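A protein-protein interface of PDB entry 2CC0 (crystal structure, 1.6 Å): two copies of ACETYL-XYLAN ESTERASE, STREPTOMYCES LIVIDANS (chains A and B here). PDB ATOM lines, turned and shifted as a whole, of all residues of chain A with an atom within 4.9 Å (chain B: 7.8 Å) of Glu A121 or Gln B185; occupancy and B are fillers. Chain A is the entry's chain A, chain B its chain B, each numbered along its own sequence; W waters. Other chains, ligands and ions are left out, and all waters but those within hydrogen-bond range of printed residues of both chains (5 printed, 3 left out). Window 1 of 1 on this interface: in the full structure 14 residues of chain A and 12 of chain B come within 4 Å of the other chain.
Of the 11 printed residues of chain B, 4 touch a printed residue of chain A. Among the printed residues, 6 pairs touch across the chains. Among the printed residues, no Asp or Glu carboxylate lies within 4 Å of a Lys or Arg side-chain nitrogen of the other chain.
The backbone NH (N) of Phe A99 lies within hydrogen-bond range of the backbone carbonyl oxygen (O) of Thr A120. OG1 of Thr A106 sits at hydrogen-bond distance from OE1 of Glu A121. NE of Arg A111 lies within salt-bridge range of OE2 of Glu A121, at 2.9 Å. The side-chain carboxylate (OE2) of Glu A114 sits close to the side-chain carboxylate (OE1) of Glu A121 (2.5 Å). The backbone NH (N) of Thr B120 is in hydrogen-bond range of the backbone carbonyl oxygen (O) of Lys B97. The backbone carbonyl oxygen of Pro B184 lies within hydrogen-bond range of the side-chain hydroxyl of Thr B120 (2.5 Å).
Glu A121 touches Gln B185 (OE2 to O, 3.7 Å).
Of the printed residues of chain B, Glu A121 touches Gln B185. Printed residues of chain A within 4 Å of Gln B185: Thr A106, Arg A111 and Glu A121. Of the printed residues of chain B, Thr A120 touches Arg B111 (2.9 Å). Printed residues of chain A within 4 Å of Pro B184: Arg A111 (3.1 Å). Of the printed residues of chain A, Thr B120 touches Arg A111 (3.0 Å). Printed residues of chain B within 4 Å of Arg A111: Thr B120 (3.0 Å), Pro B184 (3.1 Å) and Gln B185 (3.1 Å). Of the printed residues of chain B, Thr A106 touches Gln B185. The nearest printed residue of chain A that does not touch Arg B111 is Leu A119 (4.1 Å).
The backbone carbonyl oxygen (O) of Thr A106 is in hydrogen-bond range of the side-chain amide nitrogen (NE2) of Gln B185, 3.3 Å away. The guanidinium group of Arg A111 sits at hydrogen-bond distance from the side-chain hydroxyl of Thr B120. The guanidinium group (NH2) of Arg A111 sits at hydrogen-bond distance from the backbone carbonyl oxygen (O) of Pro B184 (3.1 Å). NH2 of Arg A111 is in hydrogen-bond range of O of Gln B185 (3.1 Å). OG1 of Thr A120 lies within hydrogen-bond range of NH1 of Arg B111 (2.9 Å).
Arg A111 touches Thr B120, and with the chains exchanged Thr A120 touches Arg B111. Positions printed for both chains: 111 and 120. Of the 6 pairs that touch across the chains among the printed residues, 2 have their exchanged pair printed and touching as well.
Water W2 lies within hydrogen-bond range of NE2 of Gln B185 (2.6 Å) and N of Thr A106 (3.0 Å). Water W3 lies within hydrogen-bond range of O of Thr A106 (2.8 Å) and NE2 of Gln B185 (3.0 Å). Water W5 lies within hydrogen-bond range of the side-chain carboxylate of Glu A121 (2.8 Å) and the backbone carbonyl oxygen of Gln B185 (2.9 Å). Water W4 lies within hydrogen-bond range of the backbone NH of Ile A123 (2.9 Å), the guanidinium group of Arg B188 (3.0 Å) and the backbone carbonyl oxygen of Glu A121 (3.5 Å). Water W1 lies within hydrogen-bond range of OE1 of Gln B185 (3.3 Å) and OG1 of Thr A106 (3.4 Å).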
ATOM      1  N   PHE A  99       9.846 -18.410  -7.774  1.00  0.00           N
ATOM      2  CA  PHE A  99       9.467 -17.009  -7.879  1.00  0.00           C
ATOM      3  C   PHE A  99       8.817 -16.578  -6.585  1.00  0.00           C
ATOM      4  O   PHE A  99       7.923 -17.265  -6.080  1.00  0.00           O
ATOM      5  CB  PHE A  99       8.463 -16.838  -9.038  1.00  0.00           C
ATOM      6  CG  PHE A  99       7.826 -15.456  -9.089  1.00  0.00           C
ATOM      7  CD1 PHE A  99       8.551 -14.358  -9.556  1.00  0.00           C
ATOM      8  CD2 PHE A  99       6.508 -15.263  -8.630  1.00  0.00           C
ATOM      9  CE1 PHE A  99       7.955 -13.083  -9.572  1.00  0.00           C
ATOM     10  CE2 PHE A  99       5.905 -14.001  -8.633  1.00  0.00           C
ATOM     11  CZ  PHE A  99       6.638 -12.895  -9.119  1.00  0.00           C
ATOM     12  N   PRO A 101       6.555 -13.513  -5.116  1.00  0.00           N
ATOM     13  CA  PRO A 101       5.891 -12.273  -5.507  1.00  0.00           C
ATOM     14  C   PRO A 101       6.344 -11.140  -4.574  1.00  0.00           C
ATOM     15  O   PRO A 101       6.438 -11.333  -3.352  1.00  0.00           O
ATOM     16  CB  PRO A 101       4.406 -12.562  -5.230  1.00  0.00           C
ATOM     17  CG  PRO A 101       4.284 -14.053  -5.163  1.00  0.00           C
ATOM     18  CD  PRO A 101       5.608 -14.504  -4.565  1.00  0.00           C
ATOM     19  N   THR A 106      -0.385 -12.116  -4.402  1.00  0.00           N
ATOM     20  CA  THR A 106      -0.618 -12.990  -5.557  1.00  0.00           C
ATOM     21  C   THR A 106      -2.105 -13.069  -5.949  1.00  0.00           C
ATOM     22  O   THR A 106      -2.974 -12.686  -5.176  1.00  0.00           O
ATOM     23  CB  THR A 106       0.000 -14.395  -5.294  1.00  0.00           C
ATOM     24  OG1 THR A 106      -0.139 -15.230  -6.450  1.00  0.00           O
ATOM     25  CG2 THR A 106      -0.630 -15.069  -4.098  1.00  0.00           C
ATOM     26  N   LEU A 110      -1.472 -13.951 -11.782  1.00  0.00           N
ATOM     27  CA  LEU A 110      -0.050 -14.097 -11.498  1.00  0.00           C
ATOM     28  C   LEU A 110       0.348 -15.570 -11.526  1.00  0.00           C
ATOM     29  O   LEU A 110       1.414 -15.928 -12.077  1.00  0.00           O
ATOM     30  CB  LEU A 110       0.295 -13.483 -10.147  1.00  0.00           C
ATOM     31  CG  LEU A 110       1.801 -13.448  -9.805  1.00  0.00           C
ATOM     32  CD1 LEU A 110       2.653 -12.763 -10.879  1.00  0.00           C
ATOM     33  CD2 LEU A 110       2.008 -12.783  -8.431  1.00  0.00           C
ATOM     34  N   ARG A 111      -0.498 -16.420 -10.938  1.00  0.00           N
ATOM     35  CA  ARG A 111      -0.218 -17.863 -10.943  1.00  0.00           C
ATOM     36  C   ARG A 111      -0.091 -18.414 -12.375  1.00  0.00           C
ATOM     37  O   ARG A 111       0.757 -19.277 -12.653  1.00  0.00           O
ATOM     38  CB  ARG A 111      -1.280 -18.646 -10.142  1.00  0.00           C
ATOM     39  CG  ARG A 111      -1.317 -18.307  -8.642  1.00  0.00           C
ATOM     40  CD  ARG A 111      -0.375 -19.232  -7.831  1.00  0.00           C
ATOM     41  NE  ARG A 111      -0.402 -18.894  -6.403  1.00  0.00           N
ATOM     42  CZ  ARG A 111      -1.358 -19.292  -5.559  1.00  0.00           C
ATOM     43  NH1 ARG A 111      -2.396 -20.013  -6.020  1.00  0.00           N
ATOM     44  NH2 ARG A 111      -1.289 -18.961  -4.262  1.00  0.00           N
ATOM     45  N   GLU A 114       3.323 -17.353 -13.685  1.00  0.00           N
ATOM     46  CA  GLU A 114       4.337 -18.221 -13.077  1.00  0.00           C
ATOM     47  C   GLU A 114       4.398 -19.567 -13.798  1.00  0.00           C
ATOM     48  O   GLU A 114       5.488 -20.040 -14.143  1.00  0.00           O
ATOM     49  CB  GLU A 114       4.024 -18.491 -11.606  1.00  0.00           C
ATOM     50  CG  GLU A 114       4.117 -17.269 -10.709  1.00  0.00           C
ATOM     51  CD  GLU A 114       3.373 -17.448  -9.384  1.00  0.00           C
ATOM     52  OE1 GLU A 114       2.803 -18.540  -9.127  1.00  0.00           O
ATOM     53  OE2 GLU A 114       3.396 -16.502  -8.565  1.00  0.00           O
ATOM     54  N   LEU A 119       7.723 -21.582 -13.092  1.00  0.00           N
ATOM     55  CA  LEU A 119       8.112 -21.084 -11.770  1.00  0.00           C
ATOM     56  C   LEU A 119       7.156 -21.558 -10.668  1.00  0.00           C
ATOM     57  O   LEU A 119       5.945 -21.457 -10.802  1.00  0.00           O
ATOM     58  CB  LEU A 119       8.125 -19.545 -11.790  1.00  0.00           C
ATOM     59  CG  LEU A 119       9.223 -18.940 -12.664  1.00  0.00           C
ATOM     60  CD1 LEU A 119       8.897 -17.473 -12.966  1.00  0.00           C
ATOM     61  CD2 LEU A 119      10.631 -19.025 -12.025  1.00  0.00           C
ATOM     62  N   THR A 120       7.728 -22.038  -9.574  1.00  0.00           N
ATOM     63  CA  THR A 120       6.966 -22.348  -8.363  1.00  0.00           C
ATOM     64  C   THR A 120       6.908 -21.108  -7.485  1.00  0.00           C
ATOM     65  O   THR A 120       7.946 -20.518  -7.204  1.00  0.00           O
ATOM     66  CB  THR A 120       7.671 -23.493  -7.634  1.00  0.00           C
ATOM     67  OG1 THR A 120       7.642 -24.626  -8.517  1.00  0.00           O
ATOM     68  CG2 THR A 120       6.959 -23.863  -6.316  1.00  0.00           C
ATOM     69  N   GLU A 121       5.709 -20.732  -7.024  1.00  0.00           N
ATOM     70  CA  GLU A 121       5.587 -19.568  -6.131  1.00  0.00           C
ATOM     71  C   GLU A 121       6.072 -19.932  -4.744  1.00  0.00           C
ATOM     72  O   GLU A 121       5.689 -20.976  -4.195  1.00  0.00           O
ATOM     73  CB  GLU A 121       4.124 -19.110  -6.074  1.00  0.00           C
ATOM     74  CG  GLU A 121       3.873 -17.821  -5.335  1.00  0.00           C
ATOM     75  CD  GLU A 121       2.409 -17.468  -5.452  1.00  0.00           C
ATOM     76  OE1 GLU A 121       2.033 -16.792  -6.441  1.00  0.00           O
ATOM     77  OE2 GLU A 121       1.648 -17.898  -4.561  1.00  0.00           O
ATOM     78  N   VAL A 122       6.869 -19.046  -4.159  1.00  0.00           N
ATOM     79  CA  VAL A 122       7.427 -19.259  -2.834  1.00  0.00           C
ATOM     80  C   VAL A 122       7.150 -18.028  -1.993  1.00  0.00           C
ATOM     81  O   VAL A 122       7.691 -16.950  -2.254  1.00  0.00           O
ATOM     82  CB  VAL A 122       8.947 -19.503  -2.898  1.00  0.00           C
ATOM     83  CG1 VAL A 122       9.521 -19.641  -1.479  1.00  0.00           C
ATOM     84  CG2 VAL A 122       9.248 -20.763  -3.736  1.00  0.00           C
ATOM     85  N   ILE A 123       6.274 -18.187  -1.004  1.00  0.00           N
ATOM     86  CA  ILE A 123       6.000 -17.151  -0.018  1.00  0.00           C
ATOM     87  C   ILE A 123       6.984 -17.364   1.137  1.00  0.00           C
ATOM     88  O   ILE A 123       8.181 -17.389   0.931  1.00  0.00           O
ATOM     89  CB  ILE A 123       4.491 -17.157   0.420  1.00  0.00           C
ATOM     90  CG1 ILE A 123       3.578 -17.275  -0.809  1.00  0.00           C
ATOM     91  CG2 ILE A 123       4.144 -15.886   1.206  1.00  0.00           C
ATOM     92  CD1 ILE A 123       3.666 -16.057  -1.788  1.00  0.00           C
ATOM     93  N   LYS B  97     -11.005 -23.838  -3.559  1.00  0.00           N
ATOM     94  CA  LYS B  97      -9.873 -22.964  -3.777  1.00  0.00           C
ATOM     95  C   LYS B  97      -8.547 -23.731  -3.761  1.00  0.00           C
ATOM     96  O   LYS B  97      -7.503 -23.178  -4.130  1.00  0.00           O
ATOM     97  CB  LYS B  97      -9.859 -21.910  -2.653  1.00  0.00           C
ATOM     98  CG  LYS B  97     -11.087 -20.983  -2.681  1.00  0.00           C
ATOM     99  CD  LYS B  97     -11.307 -20.373  -4.086  1.00  0.00           C
ATOM    100  CE  LYS B  97     -10.112 -19.537  -4.604  1.00  0.00           C
ATOM    101  NZ  LYS B  97     -10.225 -19.080  -6.031  1.00  0.00           N
ATOM    102  N   LEU B  98      -8.604 -25.007  -3.328  1.00  0.00           N
ATOM    103  CA  LEU B  98      -7.396 -25.829  -3.133  1.00  0.00           C
ATOM    104  C   LEU B  98      -7.479 -27.076  -3.983  1.00  0.00           C
ATOM    105  O   LEU B  98      -8.568 -27.648  -4.150  1.00  0.00           O
ATOM    106  CB  LEU B  98      -7.272 -26.260  -1.679  1.00  0.00           C
ATOM    107  CG  LEU B  98      -7.322 -25.141  -0.633  1.00  0.00           C
ATOM    108  CD1 LEU B  98      -7.278 -25.740   0.781  1.00  0.00           C
ATOM    109  CD2 LEU B  98      -6.208 -24.112  -0.879  1.00  0.00           C
ATOM    110  N   ARG B 111       0.133 -26.950 -13.352  1.00  0.00           N
ATOM    111  CA  ARG B 111       0.062 -25.638 -12.681  1.00  0.00           C
ATOM    112  C   ARG B 111      -0.764 -24.610 -13.468  1.00  0.00           C
ATOM    113  O   ARG B 111      -1.529 -23.833 -12.867  1.00  0.00           O
ATOM    114  CB  ARG B 111       1.464 -25.108 -12.408  1.00  0.00           C
ATOM    115  CG  ARG B 111       2.296 -25.998 -11.454  1.00  0.00           C
ATOM    116  CD  ARG B 111       2.160 -25.528 -10.003  1.00  0.00           C
ATOM    117  NE  ARG B 111       2.945 -26.346  -9.070  1.00  0.00           N
ATOM    118  CZ  ARG B 111       4.242 -26.156  -8.799  1.00  0.00           C
ATOM    119  NH1 ARG B 111       4.913 -25.183  -9.411  1.00  0.00           N
ATOM    120  NH2 ARG B 111       4.876 -26.940  -7.925  1.00  0.00           N
ATOM    121  N   THR B 120      -5.166 -23.278  -5.713  1.00  0.00           N
ATOM    122  CA  THR B 120      -3.825 -23.316  -5.134  1.00  0.00           C
ATOM    123  C   THR B 120      -3.424 -24.767  -4.935  1.00  0.00           C
ATOM    124  O   THR B 120      -4.154 -25.538  -4.318  1.00  0.00           O
ATOM    125  CB  THR B 120      -3.852 -22.581  -3.769  1.00  0.00           C
ATOM    126  OG1 THR B 120      -4.202 -21.205  -4.004  1.00  0.00           O
ATOM    127  CG2 THR B 120      -2.484 -22.650  -3.051  1.00  0.00           C
ATOM    128  N   ILE B 182      -6.429 -24.177   5.356  1.00  0.00           N
ATOM    129  CA  ILE B 182      -5.249 -24.007   4.521  1.00  0.00           C
ATOM    130  C   ILE B 182      -5.439 -22.754   3.688  1.00  0.00           C
ATOM    131  O   ILE B 182      -6.441 -22.604   2.952  1.00  0.00           O
ATOM    132  CB  ILE B 182      -4.942 -25.269   3.653  1.00  0.00           C
ATOM    133  CG1 ILE B 182      -4.527 -26.431   4.587  1.00  0.00           C
ATOM    134  CG2 ILE B 182      -3.827 -24.977   2.613  1.00  0.00           C
ATOM    135  CD1 ILE B 182      -4.484 -27.799   3.923  1.00  0.00           C
ATOM    136  N   SER B 183      -4.484 -21.828   3.829  1.00  0.00           N
ATOM    137  CA  SER B 183      -4.565 -20.553   3.106  1.00  0.00           C
ATOM    138  C   SER B 183      -4.444 -20.738   1.573  1.00  0.00           C
ATOM    139  O   SER B 183      -3.461 -21.303   1.104  1.00  0.00           O
ATOM    140  CB  SER B 183      -3.390 -19.648   3.557  1.00  0.00           C
ATOM    141  OG  SER B 183      -3.314 -18.465   2.736  1.00  0.00           O
ATOM    142  N   PRO B 184      -5.398 -20.211   0.785  1.00  0.00           N
ATOM    143  CA  PRO B 184      -5.196 -20.209  -0.674  1.00  0.00           C
ATOM    144  C   PRO B 184      -4.005 -19.342  -1.124  1.00  0.00           C
ATOM    145  O   PRO B 184      -3.450 -19.598  -2.184  1.00  0.00           O
ATOM    146  CB  PRO B 184      -6.503 -19.622  -1.219  1.00  0.00           C
ATOM    147  CG  PRO B 184      -7.502 -19.889  -0.102  1.00  0.00           C
ATOM    148  CD  PRO B 184      -6.708 -19.650   1.155  1.00  0.00           C
ATOM    149  N   GLN B 185      -3.570 -18.380  -0.305  1.00  0.00           N
ATOM    150  CA  GLN B 185      -2.465 -17.550  -0.751  1.00  0.00           C
ATOM    151  C   GLN B 185      -1.123 -18.256  -0.522  1.00  0.00           C
ATOM    152  O   GLN B 185      -0.265 -18.236  -1.411  1.00  0.00           O
ATOM    153  CB  GLN B 185      -2.532 -16.145  -0.141  1.00  0.00           C
ATOM    154  CG  GLN B 185      -3.798 -15.354  -0.525  1.00  0.00           C
ATOM    155  CD  GLN B 185      -3.886 -14.900  -1.992  1.00  0.00           C
ATOM    156  OE1 GLN B 185      -3.764 -15.699  -2.928  1.00  0.00           O
ATOM    157  NE2 GLN B 185      -4.167 -13.615  -2.188  1.00  0.00           N
ATOM    158  N   THR B 186      -0.961 -18.906   0.623  1.00  0.00           N
ATOM    159  CA  THR B 186       0.357 -19.459   0.996  1.00  0.00           C
ATOM    160  C   THR B 186       0.441 -20.980   1.014  1.00  0.00           C
ATOM    161  O   THR B 186       1.552 -21.533   1.021  1.00  0.00           O
ATOM    162  CB  THR B 186       0.782 -18.992   2.417  1.00  0.00           C
ATOM    163  OG1 THR B 186      -0.105 -19.605   3.384  1.00  0.00           O
ATOM    164  CG2 THR B 186       0.730 -17.500   2.569  1.00  0.00           C
ATOM    165  N   GLY B 187      -0.710 -21.652   1.034  1.00  0.00           N
ATOM    166  CA  GLY B 187      -0.794 -23.105   1.164  1.00  0.00           C
ATOM    167  C   GLY B 187      -0.392 -23.641   2.541  1.00  0.00           C
ATOM    168  O   GLY B 187      -0.137 -24.855   2.705  1.00  0.00           O
ATOM    169  N   ARG B 188      -0.330 -22.744   3.520  1.00  0.00           N
ATOM    170  CA  ARG B 188       0.025 -23.025   4.925  1.00  0.00           C
ATOM    171  C   ARG B 188      -1.253 -23.074   5.752  1.00  0.00           C
ATOM    172  O   ARG B 188      -2.222 -22.354   5.423  1.00  0.00           O
ATOM    173  CB  ARG B 188       0.845 -21.869   5.535  1.00  0.00           C
ATOM    174  CG  ARG B 188       2.362 -21.980   5.515  1.00  0.00           C
ATOM    175  CD  ARG B 188       2.881 -21.520   4.180  1.00  0.00           C
ATOM    176  NE  ARG B 188       4.333 -21.602   4.088  1.00  0.00           N
ATOM    177  CZ  ARG B 188       5.015 -21.427   2.960  1.00  0.00           C
ATOM    178  NH1 ARG B 188       4.370 -21.150   1.830  1.00  0.00           N
ATOM    179  NH2 ARG B 188       6.340 -21.519   2.969  1.00  0.00           N
HETATM  180  O   HOH W   1      -3.232 -16.593  -6.009  1.00  0.00           O
HETATM  181  O   HOH W   2      -2.152 -12.066  -1.938  1.00  0.00           O
HETATM  182  O   HOH W   3      -5.649 -12.482  -4.531  1.00  0.00           O
HETATM  183  O   HOH W   4       4.395 -20.406  -1.027  1.00  0.00           O
HETATM  184  O   HOH W   5       1.910 -19.760  -2.516  1.00  0.00           O
